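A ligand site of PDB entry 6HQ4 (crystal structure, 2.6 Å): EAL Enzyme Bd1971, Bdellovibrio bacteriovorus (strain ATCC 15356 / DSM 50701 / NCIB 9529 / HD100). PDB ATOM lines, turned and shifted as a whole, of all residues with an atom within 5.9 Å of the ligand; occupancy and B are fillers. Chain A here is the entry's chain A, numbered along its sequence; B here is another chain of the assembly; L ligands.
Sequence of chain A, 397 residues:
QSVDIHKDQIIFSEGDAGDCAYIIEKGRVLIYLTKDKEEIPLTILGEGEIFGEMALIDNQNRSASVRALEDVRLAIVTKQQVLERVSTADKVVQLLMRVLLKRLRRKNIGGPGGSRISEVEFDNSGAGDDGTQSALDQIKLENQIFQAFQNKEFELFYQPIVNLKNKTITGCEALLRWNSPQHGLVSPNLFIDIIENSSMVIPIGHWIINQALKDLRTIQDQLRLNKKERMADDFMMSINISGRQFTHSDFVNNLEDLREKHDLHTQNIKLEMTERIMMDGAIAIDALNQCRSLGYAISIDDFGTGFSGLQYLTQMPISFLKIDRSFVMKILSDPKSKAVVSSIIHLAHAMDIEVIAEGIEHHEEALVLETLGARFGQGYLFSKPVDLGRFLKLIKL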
ATOM      1  N   PHE A  12       8.204   7.950  11.900  1.00  0.00           N
ATOM      2  CA  PHE A  12       8.347   6.513  12.115  1.00  0.00           C
ATOM      3  C   PHE A  12       8.003   6.131  13.547  1.00  0.00           C
ATOM      4  O   PHE A  12       7.948   6.979  14.439  1.00  0.00           O
ATOM      5  CB  PHE A  12       9.746   6.005  11.733  1.00  0.00           C
ATOM      6  CG  PHE A  12      10.887   6.762  12.337  1.00  0.00           C
ATOM      7  CD1 PHE A  12      11.261   6.552  13.663  1.00  0.00           C
ATOM      8  CD2 PHE A  12      11.622   7.660  11.579  1.00  0.00           C
ATOM      9  CE1 PHE A  12      12.328   7.252  14.219  1.00  0.00           C
ATOM     10  CE2 PHE A  12      12.689   8.360  12.135  1.00  0.00           C
ATOM     11  CZ  PHE A  12      13.041   8.151  13.450  1.00  0.00           C
ATOM     12  N   ILE A  31       9.762  13.158  20.313  1.00  0.00           N
ATOM     13  CA  ILE A  31      10.165  11.756  20.477  1.00  0.00           C
ATOM     14  C   ILE A  31       9.451  11.176  21.696  1.00  0.00           C
ATOM     15  O   ILE A  31       9.527  11.739  22.784  1.00  0.00           O
ATOM     16  CB  ILE A  31      11.689  11.610  20.686  1.00  0.00           C
ATOM     17  CG1 ILE A  31      12.447  12.034  19.430  1.00  0.00           C
ATOM     18  CG2 ILE A  31      12.059  10.168  21.013  1.00  0.00           C
ATOM     19  CD1 ILE A  31      12.555  13.529  19.262  1.00  0.00           C
ATOM     20  N   LEU A  42       9.759  11.886  25.627  1.00  0.00           N
ATOM     21  CA  LEU A  42      11.173  11.900  25.971  1.00  0.00           C
ATOM     22  C   LEU A  42      11.730  13.308  25.822  1.00  0.00           C
ATOM     23  O   LEU A  42      12.320  13.840  26.766  1.00  0.00           O
ATOM     24  CB  LEU A  42      11.964  10.898  25.117  1.00  0.00           C
ATOM     25  CG  LEU A  42      11.637   9.413  25.312  1.00  0.00           C
ATOM     26  CD1 LEU A  42      12.599   8.552  24.496  1.00  0.00           C
ATOM     27  CD2 LEU A  42      11.691   9.007  26.778  1.00  0.00           C
ATOM     28  N   THR A  43      11.540  13.907  24.644  1.00  0.00           N
ATOM     29  CA  THR A  43      11.899  15.319  24.437  1.00  0.00           C
ATOM     30  C   THR A  43      11.314  15.903  23.146  1.00  0.00           C
ATOM     31  O   THR A  43      10.746  15.195  22.318  1.00  0.00           O
ATOM     32  CB  THR A  43      13.435  15.530  24.438  1.00  0.00           C
ATOM     33  OG1 THR A  43      13.729  16.917  24.289  1.00  0.00           O
ATOM     34  CG2 THR A  43      14.090  14.746  23.312  1.00  0.00           C
ATOM     35  N   LEU A  45      12.641  18.035  19.851  1.00  0.00           N
ATOM     36  CA  LEU A  45      13.820  18.486  19.074  1.00  0.00           C
ATOM     37  C   LEU A  45      13.445  19.606  18.109  1.00  0.00           C
ATOM     38  O   LEU A  45      12.321  19.640  17.583  1.00  0.00           O
ATOM     39  CB  LEU A  45      14.431  17.331  18.287  1.00  0.00           C
ATOM     40  CG  LEU A  45      14.847  16.076  19.045  1.00  0.00           C
ATOM     41  CD1 LEU A  45      15.358  15.030  18.063  1.00  0.00           C
ATOM     42  CD2 LEU A  45      15.915  16.373  20.099  1.00  0.00           C
ATOM     43  N   ILE A  50      19.331  16.303  15.360  1.00  0.00           N
ATOM     44  CA  ILE A  50      19.259  15.070  14.560  1.00  0.00           C
ATOM     45  C   ILE A  50      18.385  14.016  15.240  1.00  0.00           C
ATOM     46  O   ILE A  50      18.227  14.037  16.453  1.00  0.00           O
ATOM     47  CB  ILE A  50      20.679  14.473  14.321  1.00  0.00           C
ATOM     48  CG1 ILE A  50      20.672  13.453  13.185  1.00  0.00           C
ATOM     49  CG2 ILE A  50      21.232  13.829  15.597  1.00  0.00           C
ATOM     50  CD1 ILE A  50      22.039  12.891  12.849  1.00  0.00           C
ATOM     51  N   PHE A  51      17.831  13.098  14.455  1.00  0.00           N
ATOM     52  CA  PHE A  51      17.176  11.907  14.996  1.00  0.00           C
ATOM     53  C   PHE A  51      17.118  10.774  13.981  1.00  0.00           C
ATOM     54  O   PHE A  51      17.255  10.990  12.769  1.00  0.00           O
ATOM     55  CB  PHE A  51      15.771  12.221  15.552  1.00  0.00           C
ATOM     56  CG  PHE A  51      14.805  12.718  14.510  1.00  0.00           C
ATOM     57  CD1 PHE A  51      14.724  14.080  14.215  1.00  0.00           C
ATOM     58  CD2 PHE A  51      13.979  11.845  13.835  1.00  0.00           C
ATOM     59  CE1 PHE A  51      13.837  14.544  13.252  1.00  0.00           C
ATOM     60  CE2 PHE A  51      13.096  12.300  12.872  1.00  0.00           C
ATOM     61  CZ  PHE A  51      13.026  13.656  12.585  1.00  0.00           C
ATOM     62  N   GLY A  52      16.913   9.557  14.478  1.00  0.00           N
ATOM     63  CA  GLY A  52      16.909   8.349  13.641  1.00  0.00           C
ATOM     64  C   GLY A  52      18.298   7.794  13.374  1.00  0.00           C
ATOM     65  O   GLY A  52      18.457   6.907  12.535  1.00  0.00           O
ATOM     66  N   GLU A  53      19.300   8.293  14.093  1.00  0.00           N
ATOM     67  CA  GLU A  53      20.698   7.922  13.846  1.00  0.00           C
ATOM     68  C   GLU A  53      21.126   6.631  14.557  1.00  0.00           C
ATOM     69  O   GLU A  53      22.076   5.964  14.122  1.00  0.00           O
ATOM     70  CB  GLU A  53      21.633   9.085  14.210  1.00  0.00           C
ATOM     71  CG  GLU A  53      22.073   9.169  15.675  1.00  0.00           C
ATOM     72  CD  GLU A  53      20.948   9.430  16.647  1.00  0.00           C
ATOM     73  OE1 GLU A  53      19.822   9.772  16.202  1.00  0.00           O
ATOM     74  OE2 GLU A  53      21.171   9.295  17.868  1.00  0.00           O
ATOM     75  N   MET A  54      20.448   6.291  15.656  1.00  0.00           N
ATOM     76  CA  MET A  54      20.837   5.132  16.467  1.00  0.00           C
ATOM     77  C   MET A  54      20.657   3.818  15.719  1.00  0.00           C
ATOM     78  O   MET A  54      21.561   2.976  15.706  1.00  0.00           O
ATOM     79  CB  MET A  54      20.035   5.109  17.780  1.00  0.00           C
ATOM     80  CG  MET A  54      20.298   6.297  18.689  1.00  0.00           C
ATOM     81  SD  MET A  54      19.245   6.406  20.149  1.00  0.00           S
ATOM     82  CE  MET A  54      19.576   4.836  20.943  1.00  0.00           C
ATOM     83  N   ALA A  55      19.501   3.651  15.095  1.00  0.00           N
ATOM     84  CA  ALA A  55      19.198   2.432  14.327  1.00  0.00           C
ATOM     85  C   ALA A  55      20.222   2.162  13.215  1.00  0.00           C
ATOM     86  O   ALA A  55      20.526   0.998  12.922  1.00  0.00           O
ATOM     87  CB  ALA A  55      17.797   2.520  13.732  1.00  0.00           C
ATOM     88  N   LEU A  56      20.751   3.226  12.616  1.00  0.00           N
ATOM     89  CA  LEU A  56      21.702   3.098  11.513  1.00  0.00           C
ATOM     90  C   LEU A  56      23.089   2.629  11.972  1.00  0.00           C
ATOM     91  O   LEU A  56      23.775   1.924  11.253  1.00  0.00           O
ATOM     92  CB  LEU A  56      21.856   4.428  10.779  1.00  0.00           C
ATOM     93  CG  LEU A  56      20.581   5.084  10.226  1.00  0.00           C
ATOM     94  CD1 LEU A  56      20.943   6.373   9.518  1.00  0.00           C
ATOM     95  CD2 LEU A  56      19.842   4.138   9.287  1.00  0.00           C
ATOM     96  N   GLN A  60      19.890  -1.961  14.478  1.00  0.00           N
ATOM     97  CA  GLN A  60      18.738  -2.410  15.273  1.00  0.00           C
ATOM     98  C   GLN A  60      17.540  -1.500  15.042  1.00  0.00           C
ATOM     99  O   GLN A  60      17.652  -0.467  14.397  1.00  0.00           O
ATOM    100  CB  GLN A  60      19.110  -2.474  16.757  1.00  0.00           C
ATOM    101  CG  GLN A  60      20.081  -3.586  17.084  1.00  0.00           C
ATOM    102  CD  GLN A  60      20.453  -3.626  18.550  1.00  0.00           C
ATOM    103  OE1 GLN A  60      20.942  -2.637  19.103  1.00  0.00           O
ATOM    104  NE2 GLN A  60      20.240  -4.779  19.191  1.00  0.00           N
ATOM    105  N   ASN A  61      16.392  -1.909  15.584  1.00  0.00           N
ATOM    106  CA  ASN A  61      15.128  -1.210  15.328  1.00  0.00           C
ATOM    107  C   ASN A  61      15.064   0.165  15.983  1.00  0.00           C
ATOM    108  O   ASN A  61      15.933   0.547  16.767  1.00  0.00           O
ATOM    109  CB  ASN A  61      13.946  -2.071  15.800  1.00  0.00           C
ATOM    110  CG  ASN A  61      13.858  -3.407  15.084  1.00  0.00           C
ATOM    111  OD1 ASN A  61      13.364  -4.394  15.642  1.00  0.00           O
ATOM    112  ND2 ASN A  61      14.323  -3.448  13.841  1.00  0.00           N
ATOM    113  N   ARG A  62      14.011   0.908  15.656  1.00  0.00           N
ATOM    114  CA  ARG A  62      13.777   2.238  16.200  1.00  0.00           C
ATOM    115  C   ARG A  62      13.504   2.169  17.702  1.00  0.00           C
ATOM    116  O   ARG A  62      12.539   1.524  18.129  1.00  0.00           O
ATOM    117  CB  ARG A  62      12.597   2.918  15.498  1.00  0.00           C
ATOM    118  CG  ARG A  62      12.754   3.153  14.003  1.00  0.00           C
ATOM    119  CD  ARG A  62      13.926   4.076  13.690  1.00  0.00           C
ATOM    120  NE  ARG A  62      13.875   4.579  12.316  1.00  0.00           N
ATOM    121  CZ  ARG A  62      14.830   5.286  11.723  1.00  0.00           C
ATOM    122  NH1 ARG A  62      15.949   5.579  12.373  1.00  0.00           N
ATOM    123  NH2 ARG A  62      14.690   5.690  10.467  1.00  0.00           N
ATOM    124  N   SER A  63      14.341   2.838  18.493  1.00  0.00           N
ATOM    125  CA  SER A  63      14.188   2.856  19.946  1.00  0.00           C
ATOM    126  C   SER A  63      12.984   3.671  20.430  1.00  0.00           C
ATOM    127  O   SER A  63      12.596   3.576  21.600  1.00  0.00           O
ATOM    128  CB  SER A  63      15.454   3.404  20.597  1.00  0.00           C
ATOM    129  OG  SER A  63      15.662   4.769  20.266  1.00  0.00           O
ATOM    130  N   ALA A  64      12.382   4.468  19.543  1.00  0.00           N
ATOM    131  CA  ALA A  64      11.259   5.332  19.916  1.00  0.00           C
ATOM    132  C   ALA A  64      10.435   5.732  18.701  1.00  0.00           C
ATOM    133  O   ALA A  64      10.827   5.467  17.559  1.00  0.00           O
ATOM    134  CB  ALA A  64      11.753   6.561  20.634  1.00  0.00           C
ATOM    135  N   SER A  65       9.296   6.371  18.960  1.00  0.00           N
ATOM    136  CA  SER A  65       8.460   6.924  17.895  1.00  0.00           C
ATOM    137  C   SER A  65       8.721   8.416  17.763  1.00  0.00           C
ATOM    138  O   SER A  65       9.224   9.051  18.688  1.00  0.00           O
ATOM    139  CB  SER A  65       6.984   6.668  18.192  1.00  0.00           C
ATOM    140  OG  SER A  65       6.724   5.274  18.201  1.00  0.00           O
ATOM    141  N   VAL A  66       8.370   8.977  16.599  1.00  0.00           N
ATOM    142  CA  VAL A  66       8.633  10.380  16.297  1.00  0.00           C
ATOM    143  C   VAL A  66       7.462  10.980  15.513  1.00  0.00           C
ATOM    144  O   VAL A  66       7.005  10.395  14.523  1.00  0.00           O
ATOM    145  CB  VAL A  66       9.925  10.532  15.465  1.00  0.00           C
ATOM    146  CG1 VAL A  66      10.236  12.000  15.237  1.00  0.00           C
ATOM    147  CG2 VAL A  66      11.100   9.850  16.159  1.00  0.00           C
ATOM    148  N   LEU A 104      22.108   3.992  26.461  1.00  0.00           N
ATOM    149  CA  LEU A 104      20.962   4.874  26.204  1.00  0.00           C
ATOM    150  C   LEU A 104      19.681   4.077  25.964  1.00  0.00           C
ATOM    151  O   LEU A 104      18.617   4.410  26.494  1.00  0.00           O
ATOM    152  CB  LEU A 104      21.240   5.813  25.022  1.00  0.00           C
ATOM    153  CG  LEU A 104      20.235   6.955  24.817  1.00  0.00           C
ATOM    154  CD1 LEU A 104      20.258   7.925  25.991  1.00  0.00           C
ATOM    155  CD2 LEU A 104      20.524   7.694  23.522  1.00  0.00           C
ATOM    156  N   ARG A 105      19.797   3.019  25.159  1.00  0.00           N
ATOM    157  CA  ARG A 105      18.669   2.123  24.884  1.00  0.00           C
ATOM    158  C   ARG A 105      18.088   1.551  26.174  1.00  0.00           C
ATOM    159  O   ARG A 105      16.883   1.595  26.396  1.00  0.00           O
ATOM    160  CB  ARG A 105      19.089   0.982  23.947  1.00  0.00           C
ATOM    161  CG  ARG A 105      19.209   1.386  22.491  1.00  0.00           C
ATOM    162  CD  ARG A 105      19.625   0.204  21.628  1.00  0.00           C
ATOM    163  NE  ARG A 105      19.960   0.611  20.255  1.00  0.00           N
ATOM    164  CZ  ARG A 105      19.093   0.729  19.247  1.00  0.00           C
ATOM    165  NH1 ARG A 105      17.803   0.463  19.419  1.00  0.00           N
ATOM    166  NH2 ARG A 105      19.530   1.109  18.059  1.00  0.00           N
ATOM    167  N   LYS A 107      18.574   2.763  29.156  1.00  0.00           N
ATOM    168  CA  LYS A 107      18.193   3.883  30.038  1.00  0.00           C
ATOM    169  C   LYS A 107      16.717   4.260  29.934  1.00  0.00           C
ATOM    170  O   LYS A 107      15.980   4.156  30.914  1.00  0.00           O
ATOM    171  CB  LYS A 107      19.075   5.106  29.745  1.00  0.00           C
ATOM    172  CG  LYS A 107      18.940   6.243  30.746  1.00  0.00           C
ATOM    173  CD  LYS A 107      18.367   7.509  30.132  1.00  0.00           C
ATOM    174  CE  LYS A 107      18.279   8.623  31.158  1.00  0.00           C
ATOM    175  NZ  LYS A 107      18.636   9.957  30.586  1.00  0.00           N
ATOM    176  N   ASN A 108      16.278   4.698  28.747  1.00  0.00           N
ATOM    177  CA  ASN A 108      14.898   5.174  28.571  1.00  0.00           C
ATOM    178  C   ASN A 108      13.778   4.093  28.602  1.00  0.00           C
ATOM    179  O   ASN A 108      12.593   4.435  28.567  1.00  0.00           O
ATOM    180  CB  ASN A 108      14.745   6.120  27.354  1.00  0.00           C
ATOM    181  CG  ASN A 108      15.220   5.528  26.027  1.00  0.00           C
ATOM    182  OD1 ASN A 108      15.479   4.326  25.952  1.00  0.00           O
ATOM    183  ND2 ASN A 108      15.364   6.344  24.995  1.00  0.00           N
ATOM    184  N   ARG B 103      22.081  12.895  25.839  1.00  0.00           N
ATOM    185  CA  ARG B 103      20.854  12.140  26.059  1.00  0.00           C
ATOM    186  C   ARG B 103      20.983  11.100  27.158  1.00  0.00           C
ATOM    187  O   ARG B 103      20.027  10.877  27.907  1.00  0.00           O
ATOM    188  CB  ARG B 103      20.385  11.491  24.756  1.00  0.00           C
ATOM    189  CG  ARG B 103      19.988  12.515  23.708  1.00  0.00           C
ATOM    190  CD  ARG B 103      19.852  11.929  22.326  1.00  0.00           C
ATOM    191  NE  ARG B 103      19.441  12.941  21.361  1.00  0.00           N
ATOM    192  CZ  ARG B 103      19.248  12.724  20.067  1.00  0.00           C
ATOM    193  NH1 ARG B 103      19.440  11.518  19.541  1.00  0.00           N
ATOM    194  NH2 ARG B 103      18.874  13.733  19.273  1.00  0.00           N
HETATM  195  P1  LIG L   1      16.364   5.607  16.555  1.00  0.00           P
HETATM  196  O1  LIG L   1      16.691   4.612  17.640  1.00  0.00           O
HETATM  197  O2  LIG L   1      16.742   5.252  15.132  1.00  0.00           O
HETATM  198  O3  LIG L   1      14.783   5.896  16.648  1.00  0.00           O
HETATM  199  C1  LIG L   1      14.205   6.761  17.645  1.00  0.00           C
HETATM  200  C2  LIG L   1      15.036   8.036  17.720  1.00  0.00           C
HETATM  201  O4  LIG L   1      14.673   8.952  18.763  1.00  0.00           O
HETATM  202  C3  LIG L   1      16.466   7.667  18.019  1.00  0.00           C
HETATM  203  O5  LIG L   1      17.013   7.043  16.872  1.00  0.00           O
HETATM  204  C4  LIG L   1      17.038   8.975  18.501  1.00  0.00           C
HETATM  205  O6  LIG L   1      17.422   9.815  17.422  1.00  0.00           O
HETATM  206  C5  LIG L   1      15.862   9.595  19.257  1.00  0.00           C
HETATM  207  N1  LIG L   1      15.977   9.334  20.710  1.00  0.00           N
HETATM  208  C6  LIG L   1      15.961   8.118  21.293  1.00  0.00           C
HETATM  209  N2  LIG L   1      16.082   8.215  22.639  1.00  0.00           N
HETATM  210  C7  LIG L   1      16.182   9.518  22.934  1.00  0.00           C
HETATM  211  C8  LIG L   1      16.335  10.315  24.167  1.00  0.00           C
HETATM  212  N3  LIG L   1      16.402   9.696  25.368  1.00  0.00           N
HETATM  213  N4  LIG L   1      16.406  11.663  24.059  1.00  0.00           N
HETATM  214  C9  LIG L   1      16.337  12.268  22.864  1.00  0.00           C
HETATM  215  N5  LIG L   1      16.202  11.601  21.695  1.00  0.00           N
HETATM  216  C10 LIG L   1      16.121  10.256  21.665  1.00  0.00           C
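The side-chain carboxylate (OE1) of Glu 53 sits at hydrogen-bond distance from an oxygen (O6) of the ligand (2.7 Å). The backbone NH (N) of Ser 63 is in hydrogen-bond range of an oxygen (O1) of the ligand (3.1 Å). O1 of the ligand sits at hydrogen-bond distance from OG of Ser 63, 2.8 Å away. The guanidinium group (NH1) of Arg 62 is in salt-bridge range of an oxygen (O2) of the ligand, at 2.9 Å. O6 of the ligand sits at hydrogen-bond distance from N of Gly 52 (3.0 Å). A nitrogen (N2) of the ligand lies within hydrogen-bond range of the side-chain amide nitrogen (ND2) of Asn 108 (3.1 Å). N of Ala 55 is in hydrogen-bond range of O2 of the ligand (3.2 Å). The guanidinium group (NH1) of Arg 103 of chain B is in hydrogen-bond range of an oxygen (O6) of the ligand.
The guanidinium group (NH1) of Arg 103 of chain B lies within salt-bridge range of the side-chain carboxylate (OE2) of Glu 53 (3.3 Å). The guanidinium group (NH1) of Arg 62 is in hydrogen-bond range of the backbone carbonyl oxygen (O) of Gly 52 (2.8 Å). The side-chain amide oxygen of Asn 108 sits close to the backbone carbonyl oxygen of Leu 104, 3.2 Å away. OD1 of Asn 108 lies close to O of Arg 105 (3.1 Å). The backbone NH of Ile 31 is in hydrogen-bond range of the backbone carbonyl oxygen of Thr 43. NH2 of Arg 103 of chain B is in hydrogen-bond range of O of Ile 50 (2.9 Å). NZ of Lys 107 is in hydrogen-bond range of O of Arg 103 of chain B. The backbone carbonyl oxygen (O) of Phe 12 sits at hydrogen-bond distance from the backbone NH (N) of Val 66 (3.0 Å).
CE1 of Phe 12 touches O3 of the ligand (3.7 Å). Ile 31 touches the ligand. CD1 of Leu 42 touches N2 of the ligand (3.96 Å). CG2 of Thr 43 touches C9 of the ligand (3.4 Å). Phe 51 touches the ligand (CA to O6, 3.2 Å). Met 54 touches the ligand. Ala 64 touches the ligand. Hydrophobic or aromatic side chains within 4 Å of the ligand: Phe 12, Ile 31, Leu 42, Phe 51, Met 54, Ala 55 and Ala 64. Of the 24 residues printed, 14 come within 4 Å of the ligand. The nearest printed residue that does not touch the ligand is Asn 61 (4.2 Å).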
